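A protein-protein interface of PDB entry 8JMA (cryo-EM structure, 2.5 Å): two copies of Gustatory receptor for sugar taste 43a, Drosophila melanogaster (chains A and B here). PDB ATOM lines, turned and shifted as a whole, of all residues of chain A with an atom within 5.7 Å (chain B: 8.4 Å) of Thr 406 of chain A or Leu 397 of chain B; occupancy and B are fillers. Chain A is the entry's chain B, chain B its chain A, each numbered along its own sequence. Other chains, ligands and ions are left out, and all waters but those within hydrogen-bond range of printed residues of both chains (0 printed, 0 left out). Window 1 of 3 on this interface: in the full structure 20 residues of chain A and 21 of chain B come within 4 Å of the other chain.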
ATOM      1  N   ARG A 402     -19.985  22.451  -8.221  1.00  0.00           N
ATOM      2  CA  ARG A 402     -20.639  23.632  -8.767  1.00  0.00           C
ATOM      3  C   ARG A 402     -21.769  24.144  -7.884  1.00  0.00           C
ATOM      4  O   ARG A 402     -22.090  25.333  -7.947  1.00  0.00           O
ATOM      5  CB  ARG A 402     -21.160  23.331 -10.165  1.00  0.00           C
ATOM      6  CG  ARG A 402     -20.180  23.686 -11.248  1.00  0.00           C
ATOM      7  CD  ARG A 402     -20.733  23.364 -12.602  1.00  0.00           C
ATOM      8  NE  ARG A 402     -19.688  23.325 -13.612  1.00  0.00           N
ATOM      9  CZ  ARG A 402     -19.880  22.956 -14.868  1.00  0.00           C
ATOM     10  NH1 ARG A 402     -21.072  22.594 -15.308  1.00  0.00           N
ATOM     11  NH2 ARG A 402     -18.849  22.950 -15.705  1.00  0.00           N
ATOM     12  N   THR A 403     -22.368  23.287  -7.057  1.00  0.00           N
ATOM     13  CA  THR A 403     -23.423  23.755  -6.165  1.00  0.00           C
ATOM     14  C   THR A 403     -22.919  24.854  -5.240  1.00  0.00           C
ATOM     15  O   THR A 403     -23.694  25.735  -4.848  1.00  0.00           O
ATOM     16  CB  THR A 403     -23.985  22.588  -5.351  1.00  0.00           C
ATOM     17  OG1 THR A 403     -22.957  22.032  -4.526  1.00  0.00           O
ATOM     18  CG2 THR A 403     -24.528  21.512  -6.269  1.00  0.00           C
ATOM     19  N   ILE A 404     -21.625  24.845  -4.914  1.00  0.00           N
ATOM     20  CA  ILE A 404     -21.052  25.915  -4.101  1.00  0.00           C
ATOM     21  C   ILE A 404     -21.362  27.265  -4.723  1.00  0.00           C
ATOM     22  O   ILE A 404     -21.765  28.207  -4.030  1.00  0.00           O
ATOM     23  CB  ILE A 404     -19.533  25.704  -3.926  1.00  0.00           C
ATOM     24  CG1 ILE A 404     -19.275  24.744  -2.760  1.00  0.00           C
ATOM     25  CG2 ILE A 404     -18.811  27.046  -3.739  1.00  0.00           C
ATOM     26  CD1 ILE A 404     -17.842  24.678  -2.308  1.00  0.00           C
ATOM     27  N   LEU A 405     -21.203  27.377  -6.043  1.00  0.00           N
ATOM     28  CA  LEU A 405     -21.523  28.629  -6.715  1.00  0.00           C
ATOM     29  C   LEU A 405     -22.920  29.093  -6.334  1.00  0.00           C
ATOM     30  O   LEU A 405     -23.109  30.225  -5.875  1.00  0.00           O
ATOM     31  CB  LEU A 405     -21.404  28.457  -8.229  1.00  0.00           C
ATOM     32  CG  LEU A 405     -20.062  27.943  -8.752  1.00  0.00           C
ATOM     33  CD1 LEU A 405     -20.163  27.604 -10.225  1.00  0.00           C
ATOM     34  CD2 LEU A 405     -18.966  28.963  -8.506  1.00  0.00           C
ATOM     35  N   THR A 406     -23.904  28.201  -6.449  1.00  0.00           N
ATOM     36  CA  THR A 406     -25.262  28.552  -6.051  1.00  0.00           C
ATOM     37  C   THR A 406     -25.277  29.086  -4.629  1.00  0.00           C
ATOM     38  O   THR A 406     -25.765  30.193  -4.372  1.00  0.00           O
ATOM     39  CB  THR A 406     -26.178  27.337  -6.181  1.00  0.00           C
ATOM     40  OG1 THR A 406     -25.920  26.672  -7.422  1.00  0.00           O
ATOM     41  CG2 THR A 406     -27.634  27.757  -6.129  1.00  0.00           C
ATOM     42  N   SER A 407     -24.694  28.334  -3.695  1.00  0.00           N
ATOM     43  CA  SER A 407     -24.625  28.806  -2.320  1.00  0.00           C
ATOM     44  C   SER A 407     -24.023  30.198  -2.276  1.00  0.00           C
ATOM     45  O   SER A 407     -24.636  31.139  -1.757  1.00  0.00           O
ATOM     46  CB  SER A 407     -23.806  27.838  -1.469  1.00  0.00           C
ATOM     47  OG  SER A 407     -24.498  26.621  -1.273  1.00  0.00           O
ATOM     48  N   PHE A 408     -22.856  30.367  -2.901  1.00  0.00           N
ATOM     49  CA  PHE A 408     -22.225  31.677  -2.913  1.00  0.00           C
ATOM     50  C   PHE A 408     -23.207  32.717  -3.414  1.00  0.00           C
ATOM     51  O   PHE A 408     -23.489  33.707  -2.727  1.00  0.00           O
ATOM     52  CB  PHE A 408     -20.970  31.652  -3.785  1.00  0.00           C
ATOM     53  CG  PHE A 408     -19.720  31.295  -3.038  1.00  0.00           C
ATOM     54  CD1 PHE A 408     -19.735  30.312  -2.068  1.00  0.00           C
ATOM     55  CD2 PHE A 408     -18.529  31.939  -3.309  1.00  0.00           C
ATOM     56  CE1 PHE A 408     -18.590  29.984  -1.386  1.00  0.00           C
ATOM     57  CE2 PHE A 408     -17.383  31.609  -2.628  1.00  0.00           C
ATOM     58  CZ  PHE A 408     -17.415  30.629  -1.668  1.00  0.00           C
ATOM     59  N   ALA A 409     -23.817  32.455  -4.572  1.00  0.00           N
ATOM     60  CA  ALA A 409     -24.750  33.419  -5.130  1.00  0.00           C
ATOM     61  C   ALA A 409     -25.791  33.786  -4.089  1.00  0.00           C
ATOM     62  O   ALA A 409     -25.940  34.960  -3.729  1.00  0.00           O
ATOM     63  CB  ALA A 409     -25.409  32.847  -6.384  1.00  0.00           C
ATOM     64  N   SER A 410     -26.441  32.773  -3.514  1.00  0.00           N
ATOM     65  CA  SER A 410     -27.432  33.025  -2.480  1.00  0.00           C
ATOM     66  C   SER A 410     -26.861  33.968  -1.435  1.00  0.00           C
ATOM     67  O   SER A 410     -27.331  35.101  -1.272  1.00  0.00           O
ATOM     68  CB  SER A 410     -27.874  31.705  -1.850  1.00  0.00           C
ATOM     69  OG  SER A 410     -29.226  31.760  -1.446  1.00  0.00           O
ATOM     70  N   ALA A 411     -25.774  33.546  -0.786  1.00  0.00           N
ATOM     71  CA  ALA A 411     -25.188  34.363   0.264  1.00  0.00           C
ATOM     72  C   ALA A 411     -24.935  35.765  -0.250  1.00  0.00           C
ATOM     73  O   ALA A 411     -25.429  36.746   0.318  1.00  0.00           O
ATOM     74  CB  ALA A 411     -23.896  33.726   0.770  1.00  0.00           C
ATOM     75  N   GLY B 293     -29.051  23.220 -20.059  1.00  0.00           N
ATOM     76  CA  GLY B 293     -28.942  23.471 -18.637  1.00  0.00           C
ATOM     77  C   GLY B 293     -28.627  24.917 -18.330  1.00  0.00           C
ATOM     78  O   GLY B 293     -29.125  25.472 -17.354  1.00  0.00           O
ATOM     79  N   ILE B 294     -27.790  25.545 -19.154  1.00  0.00           N
ATOM     80  CA  ILE B 294     -27.483  26.953 -18.951  1.00  0.00           C
ATOM     81  C   ILE B 294     -28.716  27.806 -19.225  1.00  0.00           C
ATOM     82  O   ILE B 294     -28.999  28.767 -18.497  1.00  0.00           O
ATOM     83  CB  ILE B 294     -26.280  27.360 -19.825  1.00  0.00           C
ATOM     84  CG1 ILE B 294     -25.758  28.736 -19.416  1.00  0.00           C
ATOM     85  CG2 ILE B 294     -26.645  27.339 -21.291  1.00  0.00           C
ATOM     86  CD1 ILE B 294     -24.982  28.721 -18.123  1.00  0.00           C
ATOM     87  N   LEU B 297     -30.949  27.333 -16.237  1.00  0.00           N
ATOM     88  CA  LEU B 297     -30.418  28.064 -15.097  1.00  0.00           C
ATOM     89  C   LEU B 297     -30.732  29.546 -15.207  1.00  0.00           C
ATOM     90  O   LEU B 297     -31.138  30.178 -14.227  1.00  0.00           O
ATOM     91  CB  LEU B 297     -28.911  27.845 -14.997  1.00  0.00           C
ATOM     92  CG  LEU B 297     -28.222  28.483 -13.793  1.00  0.00           C
ATOM     93  CD1 LEU B 297     -28.623  27.778 -12.511  1.00  0.00           C
ATOM     94  CD2 LEU B 297     -26.720  28.453 -13.976  1.00  0.00           C
ATOM     95  N   LEU B 300     -34.356  30.138 -14.558  1.00  0.00           N
ATOM     96  CA  LEU B 300     -34.636  30.123 -13.126  1.00  0.00           C
ATOM     97  C   LEU B 300     -34.191  31.418 -12.465  1.00  0.00           C
ATOM     98  O   LEU B 300     -34.899  31.965 -11.610  1.00  0.00           O
ATOM     99  CB  LEU B 300     -33.942  28.929 -12.473  1.00  0.00           C
ATOM    100  CG  LEU B 300     -34.465  27.557 -12.889  1.00  0.00           C
ATOM    101  CD1 LEU B 300     -33.431  26.485 -12.613  1.00  0.00           C
ATOM    102  CD2 LEU B 300     -35.761  27.251 -12.179  1.00  0.00           C
ATOM    103  N   VAL B 301     -33.008  31.910 -12.830  1.00  0.00           N
ATOM    104  CA  VAL B 301     -32.525  33.175 -12.291  1.00  0.00           C
ATOM    105  C   VAL B 301     -33.474  34.301 -12.674  1.00  0.00           C
ATOM    106  O   VAL B 301     -33.807  35.164 -11.854  1.00  0.00           O
ATOM    107  CB  VAL B 301     -31.092  33.449 -12.784  1.00  0.00           C
ATOM    108  CG1 VAL B 301     -30.680  34.873 -12.460  1.00  0.00           C
ATOM    109  CG2 VAL B 301     -30.124  32.457 -12.173  1.00  0.00           C
ATOM    110  N   PHE B 392     -32.831  16.148 -13.600  1.00  0.00           N
ATOM    111  CA  PHE B 392     -32.319  17.139 -14.535  1.00  0.00           C
ATOM    112  C   PHE B 392     -31.439  18.129 -13.783  1.00  0.00           C
ATOM    113  O   PHE B 392     -31.839  18.664 -12.745  1.00  0.00           O
ATOM    114  CB  PHE B 392     -33.474  17.865 -15.228  1.00  0.00           C
ATOM    115  CG  PHE B 392     -33.039  18.965 -16.161  1.00  0.00           C
ATOM    116  CD1 PHE B 392     -32.615  20.189 -15.673  1.00  0.00           C
ATOM    117  CD2 PHE B 392     -33.069  18.779 -17.529  1.00  0.00           C
ATOM    118  CE1 PHE B 392     -32.216  21.193 -16.526  1.00  0.00           C
ATOM    119  CE2 PHE B 392     -32.679  19.785 -18.385  1.00  0.00           C
ATOM    120  CZ  PHE B 392     -32.251  20.990 -17.885  1.00  0.00           C
ATOM    121  N   SER B 393     -30.250  18.380 -14.312  1.00  0.00           N
ATOM    122  CA  SER B 393     -29.286  19.282 -13.699  1.00  0.00           C
ATOM    123  C   SER B 393     -29.116  20.514 -14.572  1.00  0.00           C
ATOM    124  O   SER B 393     -28.879  20.395 -15.777  1.00  0.00           O
ATOM    125  CB  SER B 393     -27.939  18.588 -13.501  1.00  0.00           C
ATOM    126  OG  SER B 393     -27.104  19.340 -12.640  1.00  0.00           O
ATOM    127  N   ALA B 394     -29.239  21.692 -13.963  1.00  0.00           N
ATOM    128  CA  ALA B 394     -28.987  22.954 -14.655  1.00  0.00           C
ATOM    129  C   ALA B 394     -27.518  23.320 -14.463  1.00  0.00           C
ATOM    130  O   ALA B 394     -27.146  24.133 -13.615  1.00  0.00           O
ATOM    131  CB  ALA B 394     -29.917  24.044 -14.141  1.00  0.00           C
ATOM    132  N   CYS B 395     -26.668  22.692 -15.275  1.00  0.00           N
ATOM    133  CA  CYS B 395     -25.227  22.931 -15.309  1.00  0.00           C
ATOM    134  C   CYS B 395     -24.522  22.482 -14.038  1.00  0.00           C
ATOM    135  O   CYS B 395     -23.403  22.923 -13.766  1.00  0.00           O
ATOM    136  CB  CYS B 395     -24.913  24.407 -15.566  1.00  0.00           C
ATOM    137  SG  CYS B 395     -25.445  25.013 -17.161  1.00  0.00           S
ATOM    138  N   GLY B 396     -25.142  21.615 -13.245  1.00  0.00           N
ATOM    139  CA  GLY B 396     -24.570  21.201 -11.987  1.00  0.00           C
ATOM    140  C   GLY B 396     -24.741  22.196 -10.866  1.00  0.00           C
ATOM    141  O   GLY B 396     -24.398  21.878  -9.723  1.00  0.00           O
ATOM    142  N   LEU B 397     -25.258  23.391 -11.154  1.00  0.00           N
ATOM    143  CA  LEU B 397     -25.520  24.365 -10.103  1.00  0.00           C
ATOM    144  C   LEU B 397     -26.625  23.883  -9.178  1.00  0.00           C
ATOM    145  O   LEU B 397     -26.538  24.044  -7.956  1.00  0.00           O
ATOM    146  CB  LEU B 397     -25.900  25.709 -10.721  1.00  0.00           C
ATOM    147  CG  LEU B 397     -24.787  26.600 -11.276  1.00  0.00           C
ATOM    148  CD1 LEU B 397     -24.107  27.338 -10.155  1.00  0.00           C
ATOM    149  CD2 LEU B 397     -23.777  25.808 -12.080  1.00  0.00           C
ATOM    150  N   CYS B 398     -27.671  23.289  -9.743  1.00  0.00           N
ATOM    151  CA  CYS B 398     -28.825  22.861  -8.973  1.00  0.00           C
ATOM    152  C   CYS B 398     -29.509  21.715  -9.696  1.00  0.00           C
ATOM    153  O   CYS B 398     -29.308  21.500 -10.891  1.00  0.00           O
ATOM    154  CB  CYS B 398     -29.817  24.010  -8.761  1.00  0.00           C
ATOM    155  SG  CYS B 398     -30.588  24.602 -10.280  1.00  0.00           S
ATOM    156  N   ARG B 399     -30.322  20.982  -8.947  1.00  0.00           N
ATOM    157  CA  ARG B 399     -31.195  19.961  -9.500  1.00  0.00           C
ATOM    158  C   ARG B 399     -32.579  20.564  -9.680  1.00  0.00           C
ATOM    159  O   ARG B 399     -33.111  21.191  -8.760  1.00  0.00           O
ATOM    160  CB  ARG B 399     -31.259  18.741  -8.582  1.00  0.00           C
ATOM    161  CG  ARG B 399     -30.448  17.557  -9.072  1.00  0.00           C
ATOM    162  CD  ARG B 399     -29.530  17.029  -7.989  1.00  0.00           C
ATOM    163  NE  ARG B 399     -30.283  16.489  -6.862  1.00  0.00           N
ATOM    164  CZ  ARG B 399     -29.966  16.656  -5.584  1.00  0.00           C
ATOM    165  NH1 ARG B 399     -28.895  17.341  -5.217  1.00  0.00           N
ATOM    166  NH2 ARG B 399     -30.744  16.119  -4.649  1.00  0.00           N
ATOM    167  N   VAL B 400     -33.152  20.390 -10.866  1.00  0.00           N
ATOM    168  CA  VAL B 400     -34.415  21.027 -11.213  1.00  0.00           C
ATOM    169  C   VAL B 400     -35.533  20.062 -10.836  1.00  0.00           C
ATOM    170  O   VAL B 400     -35.768  19.061 -11.508  1.00  0.00           O
ATOM    171  CB  VAL B 400     -34.467  21.419 -12.690  1.00  0.00           C
ATOM    172  CG1 VAL B 400     -35.712  22.239 -12.971  1.00  0.00           C
ATOM    173  CG2 VAL B 400     -33.225  22.200 -13.064  1.00  0.00           C
ATOM    174  N   ILE B 404     -36.918  23.213  -5.707  1.00  0.00           N
ATOM    175  CA  ILE B 404     -36.501  24.547  -6.128  1.00  0.00           C
ATOM    176  C   ILE B 404     -37.542  25.572  -5.715  1.00  0.00           C
ATOM    177  O   ILE B 404     -37.210  26.639  -5.185  1.00  0.00           O
ATOM    178  CB  ILE B 404     -36.245  24.577  -7.650  1.00  0.00           C
ATOM    179  CG1 ILE B 404     -34.821  24.094  -7.946  1.00  0.00           C
ATOM    180  CG2 ILE B 404     -36.509  25.977  -8.223  1.00  0.00           C
ATOM    181  CD1 ILE B 404     -34.354  24.341  -9.353  1.00  0.00           C
ATOM    182  N   SER B 407     -36.976  26.541  -2.245  1.00  0.00           N
ATOM    183  CA  SER B 407     -35.836  27.446  -2.197  1.00  0.00           C
ATOM    184  C   SER B 407     -36.253  28.833  -2.652  1.00  0.00           C
ATOM    185  O   SER B 407     -36.086  29.817  -1.923  1.00  0.00           O
ATOM    186  CB  SER B 407     -34.700  26.912  -3.067  1.00  0.00           C
ATOM    187  OG  SER B 407     -34.117  25.761  -2.492  1.00  0.00           O
ATOM    188  N   PHE B 408     -36.883  28.915  -3.827  1.00  0.00           N
ATOM    189  CA  PHE B 408     -37.325  30.209  -4.322  1.00  0.00           C
ATOM    190  C   PHE B 408     -38.157  30.908  -3.266  1.00  0.00           C
ATOM    191  O   PHE B 408     -37.844  32.030  -2.852  1.00  0.00           O
ATOM    192  CB  PHE B 408     -38.120  30.037  -5.615  1.00  0.00           C
ATOM    193  CG  PHE B 408     -37.281  30.089  -6.855  1.00  0.00           C
ATOM    194  CD1 PHE B 408     -36.038  29.488  -6.892  1.00  0.00           C
ATOM    195  CD2 PHE B 408     -37.736  30.736  -7.988  1.00  0.00           C
ATOM    196  CE1 PHE B 408     -35.270  29.534  -8.029  1.00  0.00           C
ATOM    197  CE2 PHE B 408     -36.968  30.781  -9.125  1.00  0.00           C
ATOM    198  CZ  PHE B 408     -35.737  30.176  -9.145  1.00  0.00           C
ATOM    199  N   TYR B 415     -35.820  38.126   0.881  1.00  0.00           N
ATOM    200  CA  TYR B 415     -35.580  39.359   0.141  1.00  0.00           C
ATOM    201  C   TYR B 415     -36.776  40.288   0.233  1.00  0.00           C
ATOM    202  O   TYR B 415     -36.614  41.496   0.398  1.00  0.00           O
ATOM    203  CB  TYR B 415     -35.289  39.070  -1.334  1.00  0.00           C
ATOM    204  CG  TYR B 415     -34.122  38.142  -1.581  1.00  0.00           C
ATOM    205  CD1 TYR B 415     -32.933  38.283  -0.879  1.00  0.00           C
ATOM    206  CD2 TYR B 415     -34.200  37.140  -2.539  1.00  0.00           C
ATOM    207  CE1 TYR B 415     -31.863  37.439  -1.109  1.00  0.00           C
ATOM    208  CE2 TYR B 415     -33.136  36.293  -2.777  1.00  0.00           C
ATOM    209  CZ  TYR B 415     -31.970  36.447  -2.060  1.00  0.00           C
ATOM    210  OH  TYR B 415     -30.909  35.605  -2.297  1.00  0.00           O
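Printed residues of chain B within 4 Å of Thr 403 of chain A: Gly 396 and Leu 397.
Of chain B, only Leu 397 comes within 4 Å of Thr 406 of chain A.
No residue of chain B comes within 4 Å of Ser 407 of chain A.
Printed residues of chain B within 4 Å of Ser 410 of chain A: Tyr 415 (3.8 Å).
The nearest printed residue of chain A that does not touch Leu 397 of chain B is Ile 404 of chain A (5.8 Å).
The nearest printed residue of chain B that does not touch Ser 410 of chain A is Ser 407 of chain B (7.1 Å).
3 positions are printed for both chains.
Among the printed residues, merely in contact across the chains: Thr 403 of chain A with Gly 396 of chain B (3.5 Å), Leu 405 of chain A with Leu 397 of chain B (3.5 Å), Arg 402 of chain A with Gly 396 of chain B (3.6 Å), Arg 402 of chain A with Leu 397 of chain B (3.6 Å), Thr 403 of chain A with Leu 397 of chain B (3.6 Å) and Ser 410 of chain A with Tyr 415 of chain B (3.8 Å).
The side-chain sulfur (SG) of Cys 395 of chain B sits close to the backbone carbonyl oxygen (O) of Gly 293 of chain B (3.7 Å).
The side-chain sulfur (SG) of Cys 395 of chain B sits at hydrogen-bond distance from the backbone NH (N) of Ile 294 of chain B.
OG of Ser 393 of chain B lies within hydrogen-bond range of N of Gly 396 of chain B, at 3.1 Å.
O of Cys 395 of chain B is in hydrogen-bond range of NH1 of Arg 402 of chain A (2.8 Å).
The backbone carbonyl oxygen (O) of Leu 397 of chain B is in hydrogen-bond range of the side-chain hydroxyl (OG1) of Thr 406 of chain A (2.8 Å).
Hydrophobic or aromatic side chains of chain B that line the printed part of chain A: Leu 397 and Tyr 415.
Of the 10 printed residues of chain A, 5 touch a printed residue of chain B.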
